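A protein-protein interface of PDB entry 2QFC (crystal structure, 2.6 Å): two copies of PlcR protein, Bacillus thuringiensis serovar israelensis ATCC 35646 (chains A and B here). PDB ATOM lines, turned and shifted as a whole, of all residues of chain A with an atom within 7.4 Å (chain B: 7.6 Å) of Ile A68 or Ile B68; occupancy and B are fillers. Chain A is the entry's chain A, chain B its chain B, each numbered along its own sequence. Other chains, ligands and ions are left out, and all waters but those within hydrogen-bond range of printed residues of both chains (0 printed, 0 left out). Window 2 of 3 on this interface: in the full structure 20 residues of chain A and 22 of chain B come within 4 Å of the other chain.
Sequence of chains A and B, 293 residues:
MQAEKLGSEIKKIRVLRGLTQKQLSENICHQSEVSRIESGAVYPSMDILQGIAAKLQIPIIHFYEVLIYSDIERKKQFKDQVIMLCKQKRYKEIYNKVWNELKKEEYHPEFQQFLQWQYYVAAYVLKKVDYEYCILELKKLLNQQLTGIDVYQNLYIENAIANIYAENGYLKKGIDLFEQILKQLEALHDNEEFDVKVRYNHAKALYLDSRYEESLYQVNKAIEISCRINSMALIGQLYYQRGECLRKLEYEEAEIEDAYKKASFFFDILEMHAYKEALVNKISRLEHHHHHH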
ATOM      1  N   ILE A  61     -19.097 -17.318 -31.259  1.00  0.00           N
ATOM      2  CA  ILE A  61     -17.903 -17.764 -30.534  1.00  0.00           C
ATOM      3  C   ILE A  61     -17.481 -19.193 -30.909  1.00  0.00           C
ATOM      4  O   ILE A  61     -16.411 -19.642 -30.501  1.00  0.00           O
ATOM      5  CB  ILE A  61     -18.105 -17.654 -28.980  1.00  0.00           C
ATOM      6  CG1 ILE A  61     -18.614 -16.261 -28.589  1.00  0.00           C
ATOM      7  CG2 ILE A  61     -16.817 -17.960 -28.223  1.00  0.00           C
ATOM      8  CD1 ILE A  61     -19.092 -16.147 -27.141  1.00  0.00           C
ATOM      9  N   HIS A  62     -18.306 -19.902 -31.685  1.00  0.00           N
ATOM     10  CA  HIS A  62     -17.946 -21.253 -32.123  1.00  0.00           C
ATOM     11  C   HIS A  62     -16.881 -21.245 -33.218  1.00  0.00           C
ATOM     12  O   HIS A  62     -16.054 -22.159 -33.289  1.00  0.00           O
ATOM     13  CB  HIS A  62     -19.160 -22.069 -32.569  1.00  0.00           C
ATOM     14  CG  HIS A  62     -18.880 -23.536 -32.683  1.00  0.00           C
ATOM     15  ND1 HIS A  62     -18.959 -24.399 -31.601  1.00  0.00           N
ATOM     16  CD2 HIS A  62     -18.500 -24.290 -33.747  1.00  0.00           C
ATOM     17  CE1 HIS A  62     -18.647 -25.620 -31.994  1.00  0.00           C
ATOM     18  NE2 HIS A  62     -18.362 -25.582 -33.292  1.00  0.00           N
ATOM     19  N   PHE A  63     -16.895 -20.217 -34.065  1.00  0.00           N
ATOM     20  CA  PHE A  63     -15.844 -20.060 -35.073  1.00  0.00           C
ATOM     21  C   PHE A  63     -14.544 -19.526 -34.474  1.00  0.00           C
ATOM     22  O   PHE A  63     -13.470 -20.017 -34.813  1.00  0.00           O
ATOM     23  CB  PHE A  63     -16.316 -19.202 -36.245  1.00  0.00           C
ATOM     24  CG  PHE A  63     -17.460 -19.811 -37.028  1.00  0.00           C
ATOM     25  CD1 PHE A  63     -17.318 -21.053 -37.643  1.00  0.00           C
ATOM     26  CD2 PHE A  63     -18.668 -19.135 -37.159  1.00  0.00           C
ATOM     27  CE1 PHE A  63     -18.350 -21.613 -38.364  1.00  0.00           C
ATOM     28  CE2 PHE A  63     -19.709 -19.689 -37.881  1.00  0.00           C
ATOM     29  CZ  PHE A  63     -19.548 -20.930 -38.487  1.00  0.00           C
ATOM     30  N   TYR A  64     -14.648 -18.535 -33.584  1.00  0.00           N
ATOM     31  CA  TYR A  64     -13.501 -18.068 -32.801  1.00  0.00           C
ATOM     32  C   TYR A  64     -12.929 -19.226 -31.992  1.00  0.00           C
ATOM     33  O   TYR A  64     -11.710 -19.443 -31.977  1.00  0.00           O
ATOM     34  CB  TYR A  64     -13.870 -16.897 -31.881  1.00  0.00           C
ATOM     35  CG  TYR A  64     -14.382 -15.667 -32.601  1.00  0.00           C
ATOM     36  CD1 TYR A  64     -13.524 -14.841 -33.335  1.00  0.00           C
ATOM     37  CD2 TYR A  64     -15.729 -15.316 -32.530  1.00  0.00           C
ATOM     38  CE1 TYR A  64     -14.007 -13.703 -33.997  1.00  0.00           C
ATOM     39  CE2 TYR A  64     -16.222 -14.187 -33.177  1.00  0.00           C
ATOM     40  CZ  TYR A  64     -15.367 -13.385 -33.910  1.00  0.00           C
ATOM     41  OH  TYR A  64     -15.895 -12.273 -34.538  1.00  0.00           O
ATOM     42  N   GLU A  65     -13.815 -19.975 -31.340  1.00  0.00           N
ATOM     43  CA  GLU A  65     -13.443 -21.224 -30.687  1.00  0.00           C
ATOM     44  C   GLU A  65     -12.623 -22.065 -31.658  1.00  0.00           C
ATOM     45  O   GLU A  65     -11.475 -22.401 -31.373  1.00  0.00           O
ATOM     46  CB  GLU A  65     -14.685 -21.989 -30.213  1.00  0.00           C
ATOM     47  CG  GLU A  65     -14.402 -23.189 -29.312  1.00  0.00           C
ATOM     48  CD  GLU A  65     -15.583 -23.534 -28.406  1.00  0.00           C
ATOM     49  OE1 GLU A  65     -16.647 -23.954 -28.932  1.00  0.00           O
ATOM     50  OE2 GLU A  65     -15.441 -23.387 -27.164  1.00  0.00           O
ATOM     51  N   VAL A  66     -13.208 -22.367 -32.812  1.00  0.00           N
ATOM     52  CA  VAL A  66     -12.515 -23.083 -33.870  1.00  0.00           C
ATOM     53  C   VAL A  66     -11.142 -22.453 -34.177  1.00  0.00           C
ATOM     54  O   VAL A  66     -10.121 -23.146 -34.172  1.00  0.00           O
ATOM     55  CB  VAL A  66     -13.397 -23.167 -35.137  1.00  0.00           C
ATOM     56  CG1 VAL A  66     -12.566 -23.243 -36.412  1.00  0.00           C
ATOM     57  CG2 VAL A  66     -14.348 -24.348 -35.036  1.00  0.00           C
ATOM     58  N   LEU A  67     -11.134 -21.143 -34.415  1.00  0.00           N
ATOM     59  CA  LEU A  67      -9.930 -20.432 -34.808  1.00  0.00           C
ATOM     60  C   LEU A  67      -8.839 -20.537 -33.744  1.00  0.00           C
ATOM     61  O   LEU A  67      -7.658 -20.739 -34.066  1.00  0.00           O
ATOM     62  CB  LEU A  67     -10.249 -18.972 -35.141  1.00  0.00           C
ATOM     63  CG  LEU A  67     -10.736 -18.753 -36.578  1.00  0.00           C
ATOM     64  CD1 LEU A  67     -11.712 -17.587 -36.700  1.00  0.00           C
ATOM     65  CD2 LEU A  67      -9.562 -18.564 -37.527  1.00  0.00           C
ATOM     66  N   ILE A  68      -9.240 -20.449 -32.476  1.00  0.00           N
ATOM     67  CA  ILE A  68      -8.266 -20.470 -31.385  1.00  0.00           C
ATOM     68  C   ILE A  68      -7.560 -21.819 -31.211  1.00  0.00           C
ATOM     69  O   ILE A  68      -6.339 -21.855 -31.038  1.00  0.00           O
ATOM     70  CB  ILE A  68      -8.863 -19.911 -30.082  1.00  0.00           C
ATOM     71  CG1 ILE A  68      -9.151 -18.418 -30.274  1.00  0.00           C
ATOM     72  CG2 ILE A  68      -7.895 -20.094 -28.927  1.00  0.00           C
ATOM     73  CD1 ILE A  68     -10.201 -17.841 -29.373  1.00  0.00           C
ATOM     74  N   TYR A  69      -8.312 -22.916 -31.287  1.00  0.00           N
ATOM     75  CA  TYR A  69      -7.728 -24.264 -31.276  1.00  0.00           C
ATOM     76  C   TYR A  69      -6.787 -24.487 -32.481  1.00  0.00           C
ATOM     77  O   TYR A  69      -5.767 -25.175 -32.375  1.00  0.00           O
ATOM     78  CB  TYR A  69      -8.824 -25.338 -31.273  1.00  0.00           C
ATOM     79  CG  TYR A  69      -9.649 -25.507 -29.980  1.00  0.00           C
ATOM     80  CD1 TYR A  69     -10.123 -24.402 -29.253  1.00  0.00           C
ATOM     81  CD2 TYR A  69      -9.995 -26.784 -29.520  1.00  0.00           C
ATOM     82  CE1 TYR A  69     -10.890 -24.566 -28.090  1.00  0.00           C
ATOM     83  CE2 TYR A  69     -10.776 -26.956 -28.356  1.00  0.00           C
ATOM     84  CZ  TYR A  69     -11.215 -25.842 -27.652  1.00  0.00           C
ATOM     85  OH  TYR A  69     -11.968 -26.004 -26.516  1.00  0.00           O
ATOM     86  N   SER A  70      -7.123 -23.891 -33.621  1.00  0.00           N
ATOM     87  CA  SER A  70      -6.377 -24.133 -34.838  1.00  0.00           C
ATOM     88  C   SER A  70      -5.072 -23.348 -34.815  1.00  0.00           C
ATOM     89  O   SER A  70      -4.060 -23.796 -35.331  1.00  0.00           O
ATOM     90  CB  SER A  70      -7.205 -23.729 -36.050  1.00  0.00           C
ATOM     91  OG  SER A  70      -7.170 -22.325 -36.208  1.00  0.00           O
ATOM     92  N   ASP A  71      -5.136 -22.166 -34.218  1.00  0.00           N
ATOM     93  CA  ASP A  71      -3.977 -21.336 -33.977  1.00  0.00           C
ATOM     94  C   ASP A  71      -3.102 -21.927 -32.865  1.00  0.00           C
ATOM     95  O   ASP A  71      -1.865 -21.956 -33.031  1.00  0.00           O
ATOM     96  CB  ASP A  71      -4.385 -19.891 -33.660  1.00  0.00           C
ATOM     97  CG  ASP A  71      -3.226 -18.920 -33.751  1.00  0.00           C
ATOM     98  OD1 ASP A  71      -2.866 -18.300 -32.724  1.00  0.00           O
ATOM     99  OD2 ASP A  71      -2.658 -18.777 -34.855  1.00  0.00           O
ATOM    100  N   ILE A  72      -3.684 -22.410 -31.753  1.00  0.00           N
ATOM    101  CA  ILE A  72      -2.784 -22.996 -30.734  1.00  0.00           C
ATOM    102  C   ILE A  72      -2.104 -24.243 -31.290  1.00  0.00           C
ATOM    103  O   ILE A  72      -0.921 -24.462 -31.044  1.00  0.00           O
ATOM    104  CB  ILE A  72      -3.348 -23.205 -29.261  1.00  0.00           C
ATOM    105  CG1 ILE A  72      -3.765 -24.647 -28.998  1.00  0.00           C
ATOM    106  CG2 ILE A  72      -4.419 -22.178 -28.880  1.00  0.00           C
ATOM    107  CD1 ILE A  72      -5.275 -24.905 -29.280  1.00  0.00           C
ATOM    108  N   GLU A  73      -2.836 -25.035 -32.066  1.00  0.00           N
ATOM    109  CA  GLU A  73      -2.252 -26.220 -32.685  1.00  0.00           C
ATOM    110  C   GLU A  73      -1.204 -25.857 -33.740  1.00  0.00           C
ATOM    111  O   GLU A  73      -0.159 -26.502 -33.827  1.00  0.00           O
ATOM    112  CB  GLU A  73      -3.333 -27.123 -33.280  1.00  0.00           C
ATOM    113  CG  GLU A  73      -3.038 -28.608 -33.101  1.00  0.00           C
ATOM    114  CD  GLU A  73      -2.676 -29.002 -31.638  1.00  0.00           C
ATOM    115  OE1 GLU A  73      -3.526 -28.864 -30.708  1.00  0.00           O
ATOM    116  OE2 GLU A  73      -1.525 -29.462 -31.431  1.00  0.00           O
ATOM    117  N   ARG A  74      -1.487 -24.821 -34.525  1.00  0.00           N
ATOM    118  CA  ARG A  74      -0.548 -24.334 -35.524  1.00  0.00           C
ATOM    119  C   ARG A  74       0.779 -24.036 -34.812  1.00  0.00           C
ATOM    120  O   ARG A  74       1.851 -24.509 -35.218  1.00  0.00           O
ATOM    121  CB  ARG A  74      -1.091 -23.052 -36.195  1.00  0.00           C
ATOM    122  CG  ARG A  74      -0.819 -22.898 -37.692  1.00  0.00           C
ATOM    123  CD  ARG A  74       0.602 -22.412 -38.009  1.00  0.00           C
ATOM    124  NE  ARG A  74       0.764 -20.949 -37.929  1.00  0.00           N
ATOM    125  CZ  ARG A  74       1.877 -20.319 -37.518  1.00  0.00           C
ATOM    126  NH1 ARG A  74       2.939 -21.015 -37.127  1.00  0.00           N
ATOM    127  NH2 ARG A  74       1.927 -18.988 -37.482  1.00  0.00           N
ATOM    128  N   ILE B  61     -12.897 -10.462 -27.320  1.00  0.00           N
ATOM    129  CA  ILE B  61     -12.328 -11.736 -27.773  1.00  0.00           C
ATOM    130  C   ILE B  61     -11.099 -12.125 -26.931  1.00  0.00           C
ATOM    131  O   ILE B  61     -10.700 -13.290 -26.914  1.00  0.00           O
ATOM    132  CB  ILE B  61     -11.943 -11.719 -29.301  1.00  0.00           C
ATOM    133  CG1 ILE B  61     -12.921 -10.870 -30.131  1.00  0.00           C
ATOM    134  CG2 ILE B  61     -11.891 -13.138 -29.856  1.00  0.00           C
ATOM    135  CD1 ILE B  61     -12.545 -10.740 -31.628  1.00  0.00           C
ATOM    136  N   HIS B  62     -10.520 -11.146 -26.227  1.00  0.00           N
ATOM    137  CA  HIS B  62      -9.302 -11.361 -25.441  1.00  0.00           C
ATOM    138  C   HIS B  62      -9.556 -12.194 -24.191  1.00  0.00           C
ATOM    139  O   HIS B  62      -8.900 -13.224 -23.992  1.00  0.00           O
ATOM    140  CB  HIS B  62      -8.634 -10.035 -25.071  1.00  0.00           C
ATOM    141  CG  HIS B  62      -7.328 -10.203 -24.354  1.00  0.00           C
ATOM    142  ND1 HIS B  62      -6.079 -10.755 -25.175  1.00  0.00           N
ATOM    143  CD2 HIS B  62      -7.065  -9.897 -22.881  1.00  0.00           C
ATOM    144  CE1 HIS B  62      -5.099 -10.773 -24.294  1.00  0.00           C
ATOM    145  NE2 HIS B  62      -5.693 -10.262 -22.816  1.00  0.00           N
ATOM    146  N   PHE B  63     -10.499 -11.762 -23.354  1.00  0.00           N
ATOM    147  CA  PHE B  63     -10.849 -12.538 -22.164  1.00  0.00           C
ATOM    148  C   PHE B  63     -11.340 -13.939 -22.539  1.00  0.00           C
ATOM    149  O   PHE B  63     -10.956 -14.930 -21.910  1.00  0.00           O
ATOM    150  CB  PHE B  63     -11.890 -11.812 -21.314  1.00  0.00           C
ATOM    151  CG  PHE B  63     -11.357 -10.595 -20.595  1.00  0.00           C
ATOM    152  CD1 PHE B  63     -10.095 -10.613 -20.000  1.00  0.00           C
ATOM    153  CD2 PHE B  63     -12.133  -9.447 -20.485  1.00  0.00           C
ATOM    154  CE1 PHE B  63      -9.606  -9.501 -19.326  1.00  0.00           C
ATOM    155  CE2 PHE B  63     -11.654  -8.323 -19.810  1.00  0.00           C
ATOM    156  CZ  PHE B  63     -10.387  -8.349 -19.231  1.00  0.00           C
ATOM    157  N   TYR B  64     -12.172 -14.011 -23.575  1.00  0.00           N
ATOM    158  CA  TYR B  64     -12.655 -15.283 -24.085  1.00  0.00           C
ATOM    159  C   TYR B  64     -11.505 -16.150 -24.556  1.00  0.00           C
ATOM    160  O   TYR B  64     -11.434 -17.325 -24.208  1.00  0.00           O
ATOM    161  CB  TYR B  64     -13.711 -15.082 -25.175  1.00  0.00           C
ATOM    162  CG  TYR B  64     -15.067 -14.748 -24.593  1.00  0.00           C
ATOM    163  CD1 TYR B  64     -15.628 -15.560 -23.598  1.00  0.00           C
ATOM    164  CD2 TYR B  64     -15.787 -13.628 -25.021  1.00  0.00           C
ATOM    165  CE1 TYR B  64     -16.866 -15.272 -23.040  1.00  0.00           C
ATOM    166  CE2 TYR B  64     -17.039 -13.327 -24.468  1.00  0.00           C
ATOM    167  CZ  TYR B  64     -17.568 -14.160 -23.473  1.00  0.00           C
ATOM    168  OH  TYR B  64     -18.798 -13.899 -22.909  1.00  0.00           O
ATOM    169  N   GLU B  65     -10.590 -15.555 -25.313  1.00  0.00           N
ATOM    170  CA  GLU B  65      -9.366 -16.233 -25.721  1.00  0.00           C
ATOM    171  C   GLU B  65      -8.642 -16.783 -24.496  1.00  0.00           C
ATOM    172  O   GLU B  65      -8.252 -17.947 -24.478  1.00  0.00           O
ATOM    173  CB  GLU B  65      -8.448 -15.287 -26.517  1.00  0.00           C
ATOM    174  CG  GLU B  65      -7.250 -15.973 -27.209  1.00  0.00           C
ATOM    175  CD  GLU B  65      -6.470 -14.989 -28.116  1.00  0.00           C
ATOM    176  OE1 GLU B  65      -5.860 -14.000 -27.585  1.00  0.00           O
ATOM    177  OE2 GLU B  65      -6.461 -15.212 -29.362  1.00  0.00           O
ATOM    178  N   VAL B  66      -8.480 -15.946 -23.476  1.00  0.00           N
ATOM    179  CA  VAL B  66      -7.838 -16.365 -22.245  1.00  0.00           C
ATOM    180  C   VAL B  66      -8.577 -17.582 -21.689  1.00  0.00           C
ATOM    181  O   VAL B  66      -7.965 -18.613 -21.407  1.00  0.00           O
ATOM    182  CB  VAL B  66      -7.805 -15.215 -21.214  1.00  0.00           C
ATOM    183  CG1 VAL B  66      -7.595 -15.718 -19.792  1.00  0.00           C
ATOM    184  CG2 VAL B  66      -6.739 -14.186 -21.597  1.00  0.00           C
ATOM    185  N   LEU B  67      -9.897 -17.444 -21.577  1.00  0.00           N
ATOM    186  CA  LEU B  67     -10.791 -18.468 -21.066  1.00  0.00           C
ATOM    187  C   LEU B  67     -10.695 -19.760 -21.897  1.00  0.00           C
ATOM    188  O   LEU B  67     -10.659 -20.865 -21.343  1.00  0.00           O
ATOM    189  CB  LEU B  67     -12.207 -17.881 -21.016  1.00  0.00           C
ATOM    190  CG  LEU B  67     -13.548 -18.568 -20.731  1.00  0.00           C
ATOM    191  CD1 LEU B  67     -13.491 -19.757 -19.748  1.00  0.00           C
ATOM    192  CD2 LEU B  67     -14.531 -17.495 -20.247  1.00  0.00           C
ATOM    193  N   ILE B  68     -10.587 -19.603 -23.215  1.00  0.00           N
ATOM    194  CA  ILE B  68     -10.442 -20.732 -24.139  1.00  0.00           C
ATOM    195  C   ILE B  68      -9.082 -21.441 -24.045  1.00  0.00           C
ATOM    196  O   ILE B  68      -9.029 -22.664 -24.113  1.00  0.00           O
ATOM    197  CB  ILE B  68     -10.742 -20.294 -25.590  1.00  0.00           C
ATOM    198  CG1 ILE B  68     -12.236 -19.983 -25.734  1.00  0.00           C
ATOM    199  CG2 ILE B  68     -10.301 -21.359 -26.580  1.00  0.00           C
ATOM    200  CD1 ILE B  68     -12.668 -19.539 -27.116  1.00  0.00           C
ATOM    201  N   TYR B  69      -7.997 -20.678 -23.891  1.00  0.00           N
ATOM    202  CA  TYR B  69      -6.661 -21.228 -23.606  1.00  0.00           C
ATOM    203  C   TYR B  69      -6.660 -21.944 -22.264  1.00  0.00           C
ATOM    204  O   TYR B  69      -5.897 -22.890 -22.061  1.00  0.00           O
ATOM    205  CB  TYR B  69      -5.616 -20.113 -23.497  1.00  0.00           C
ATOM    206  CG  TYR B  69      -4.916 -19.649 -24.765  1.00  0.00           C
ATOM    207  CD1 TYR B  69      -3.521 -19.599 -24.822  1.00  0.00           C
ATOM    208  CD2 TYR B  69      -5.637 -19.215 -25.880  1.00  0.00           C
ATOM    209  CE1 TYR B  69      -2.859 -19.133 -25.959  1.00  0.00           C
ATOM    210  CE2 TYR B  69      -4.987 -18.755 -27.026  1.00  0.00           C
ATOM    211  CZ  TYR B  69      -3.598 -18.714 -27.055  1.00  0.00           C
ATOM    212  OH  TYR B  69      -2.955 -18.273 -28.181  1.00  0.00           O
ATOM    213  N   SER B  70      -7.495 -21.473 -21.339  1.00  0.00           N
ATOM    214  CA  SER B  70      -7.498 -21.981 -19.984  1.00  0.00           C
ATOM    215  C   SER B  70      -8.184 -23.337 -19.945  1.00  0.00           C
ATOM    216  O   SER B  70      -7.752 -24.270 -19.266  1.00  0.00           O
ATOM    217  CB  SER B  70      -8.244 -21.012 -19.082  1.00  0.00           C
ATOM    218  OG  SER B  70      -7.937 -21.263 -17.725  1.00  0.00           O
ATOM    219  N   ASP B  71      -9.273 -23.409 -20.694  1.00  0.00           N
ATOM    220  CA  ASP B  71     -10.039 -24.605 -20.875  1.00  0.00           C
ATOM    221  C   ASP B  71      -9.147 -25.631 -21.552  1.00  0.00           C
ATOM    222  O   ASP B  71      -9.055 -26.768 -21.099  1.00  0.00           O
ATOM    223  CB  ASP B  71     -11.251 -24.285 -21.744  1.00  0.00           C
ATOM    224  CG  ASP B  71     -12.389 -25.243 -21.537  1.00  0.00           C
ATOM    225  OD1 ASP B  71     -12.154 -26.465 -21.558  1.00  0.00           O
ATOM    226  OD2 ASP B  71     -13.529 -24.767 -21.368  1.00  0.00           O
ATOM    227  N   ILE B  72      -8.456 -25.230 -22.614  1.00  0.00           N
ATOM    228  CA  ILE B  72      -7.689 -26.219 -23.361  1.00  0.00           C
ATOM    229  C   ILE B  72      -6.574 -26.820 -22.506  1.00  0.00           C
ATOM    230  O   ILE B  72      -6.400 -28.042 -22.481  1.00  0.00           O
ATOM    231  CB  ILE B  72      -7.242 -25.740 -24.790  1.00  0.00           C
ATOM    232  CG1 ILE B  72      -6.127 -26.617 -25.329  1.00  0.00           C
ATOM    233  CG2 ILE B  72      -6.724 -24.351 -24.758  1.00  0.00           C
ATOM    234  CD1 ILE B  72      -6.204 -26.829 -26.809  1.00  0.00           C
ATOM    235  N   GLU B  73      -5.869 -25.979 -21.762  1.00  0.00           N
ATOM    236  CA  GLU B  73      -4.853 -26.480 -20.841  1.00  0.00           C
ATOM    237  C   GLU B  73      -5.479 -27.293 -19.703  1.00  0.00           C
ATOM    238  O   GLU B  73      -4.877 -28.247 -19.219  1.00  0.00           O
ATOM    239  CB  GLU B  73      -3.989 -25.338 -20.277  1.00  0.00           C
ATOM    240  CG  GLU B  73      -2.588 -25.784 -19.821  1.00  0.00           C
ATOM    241  CD  GLU B  73      -1.628 -26.201 -20.982  1.00  0.00           C
ATOM    242  OE1 GLU B  73      -1.710 -25.655 -22.127  1.00  0.00           O
ATOM    243  OE2 GLU B  73      -0.758 -27.074 -20.735  1.00  0.00           O
ATOM    244  N   ARG B  74      -6.677 -26.900 -19.280  1.00  0.00           N
ATOM    245  CA  ARG B  74      -7.388 -27.593 -18.196  1.00  0.00           C
ATOM    246  C   ARG B  74      -7.604 -29.035 -18.628  1.00  0.00           C
ATOM    247  O   ARG B  74      -7.367 -29.976 -17.859  1.00  0.00           O
ATOM    248  CB  ARG B  74      -8.759 -26.947 -17.928  1.00  0.00           C
ATOM    249  CG  ARG B  74      -9.161 -26.818 -16.472  1.00  0.00           C
ATOM    250  CD  ARG B  74      -9.687 -28.126 -15.864  1.00  0.00           C
ATOM    251  NE  ARG B  74     -10.984 -28.535 -16.426  1.00  0.00           N
ATOM    252  CZ  ARG B  74     -11.696 -29.599 -16.032  1.00  0.00           C
ATOM    253  NH1 ARG B  74     -11.263 -30.405 -15.051  1.00  0.00           N
ATOM    254  NH2 ARG B  74     -12.861 -29.853 -16.623  1.00  0.00           N
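Ile B68 touches Ile A68. CG2 of Ile A68 touches CE2 of Tyr B69 (3.7 Å). Ile B68 touches Tyr A69 (CG2 to CE1, 3.6 Å). Ile A72 touches Tyr B69. Ile A72 touches Ile B72 (CD1 to CD1, 3.3 Å).
Of chain B, only Ile B68 (3.6 Å) and Tyr B69 (3.7 Å) come within 4 Å of Ile A68. Of chain A, only Ile A68 and Tyr A69 come within 4 Å of Ile B68. Of the printed residues of chain A, Tyr B69 touches Ile A68 and Ile A72. Printed residues of chain B within 4 Å of Tyr A69: Ile B68. Of the printed residues of chain A, Ile B72 touches Ile A72 (3.3 Å). Printed residues of chain B within 4 Å of Ile A72: Tyr B69 (3.9 Å) and Ile B72 (3.3 Å). The nearest residue of chain B that does not touch Ile A68 is Glu B65 (4.1 Å). The nearest residue of chain A that does not touch Ile B68 is Glu A65 (4.02 Å).
Ile A68 touches its own counterpart, Ile B68. Ile A68 touches Tyr B69, and with the chains exchanged Tyr A69 touches Ile B68. Ile A72 touches Tyr B69, but with the chains exchanged Tyr A69 does not touch Ile B72 (4.7 Å). Ile A72 touches its own counterpart, Ile B72.
Hydrophobic or aromatic side chains of chain B that line the printed part of chain A: Ile B68, Tyr B69 and Ile B72. Of the 14 printed residues of chain A, 3 touch a printed residue of chain B. Hydrophobic or aromatic side chains of chain A that line the printed part of chain B: Ile A68, Tyr A69 and Ile A72.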
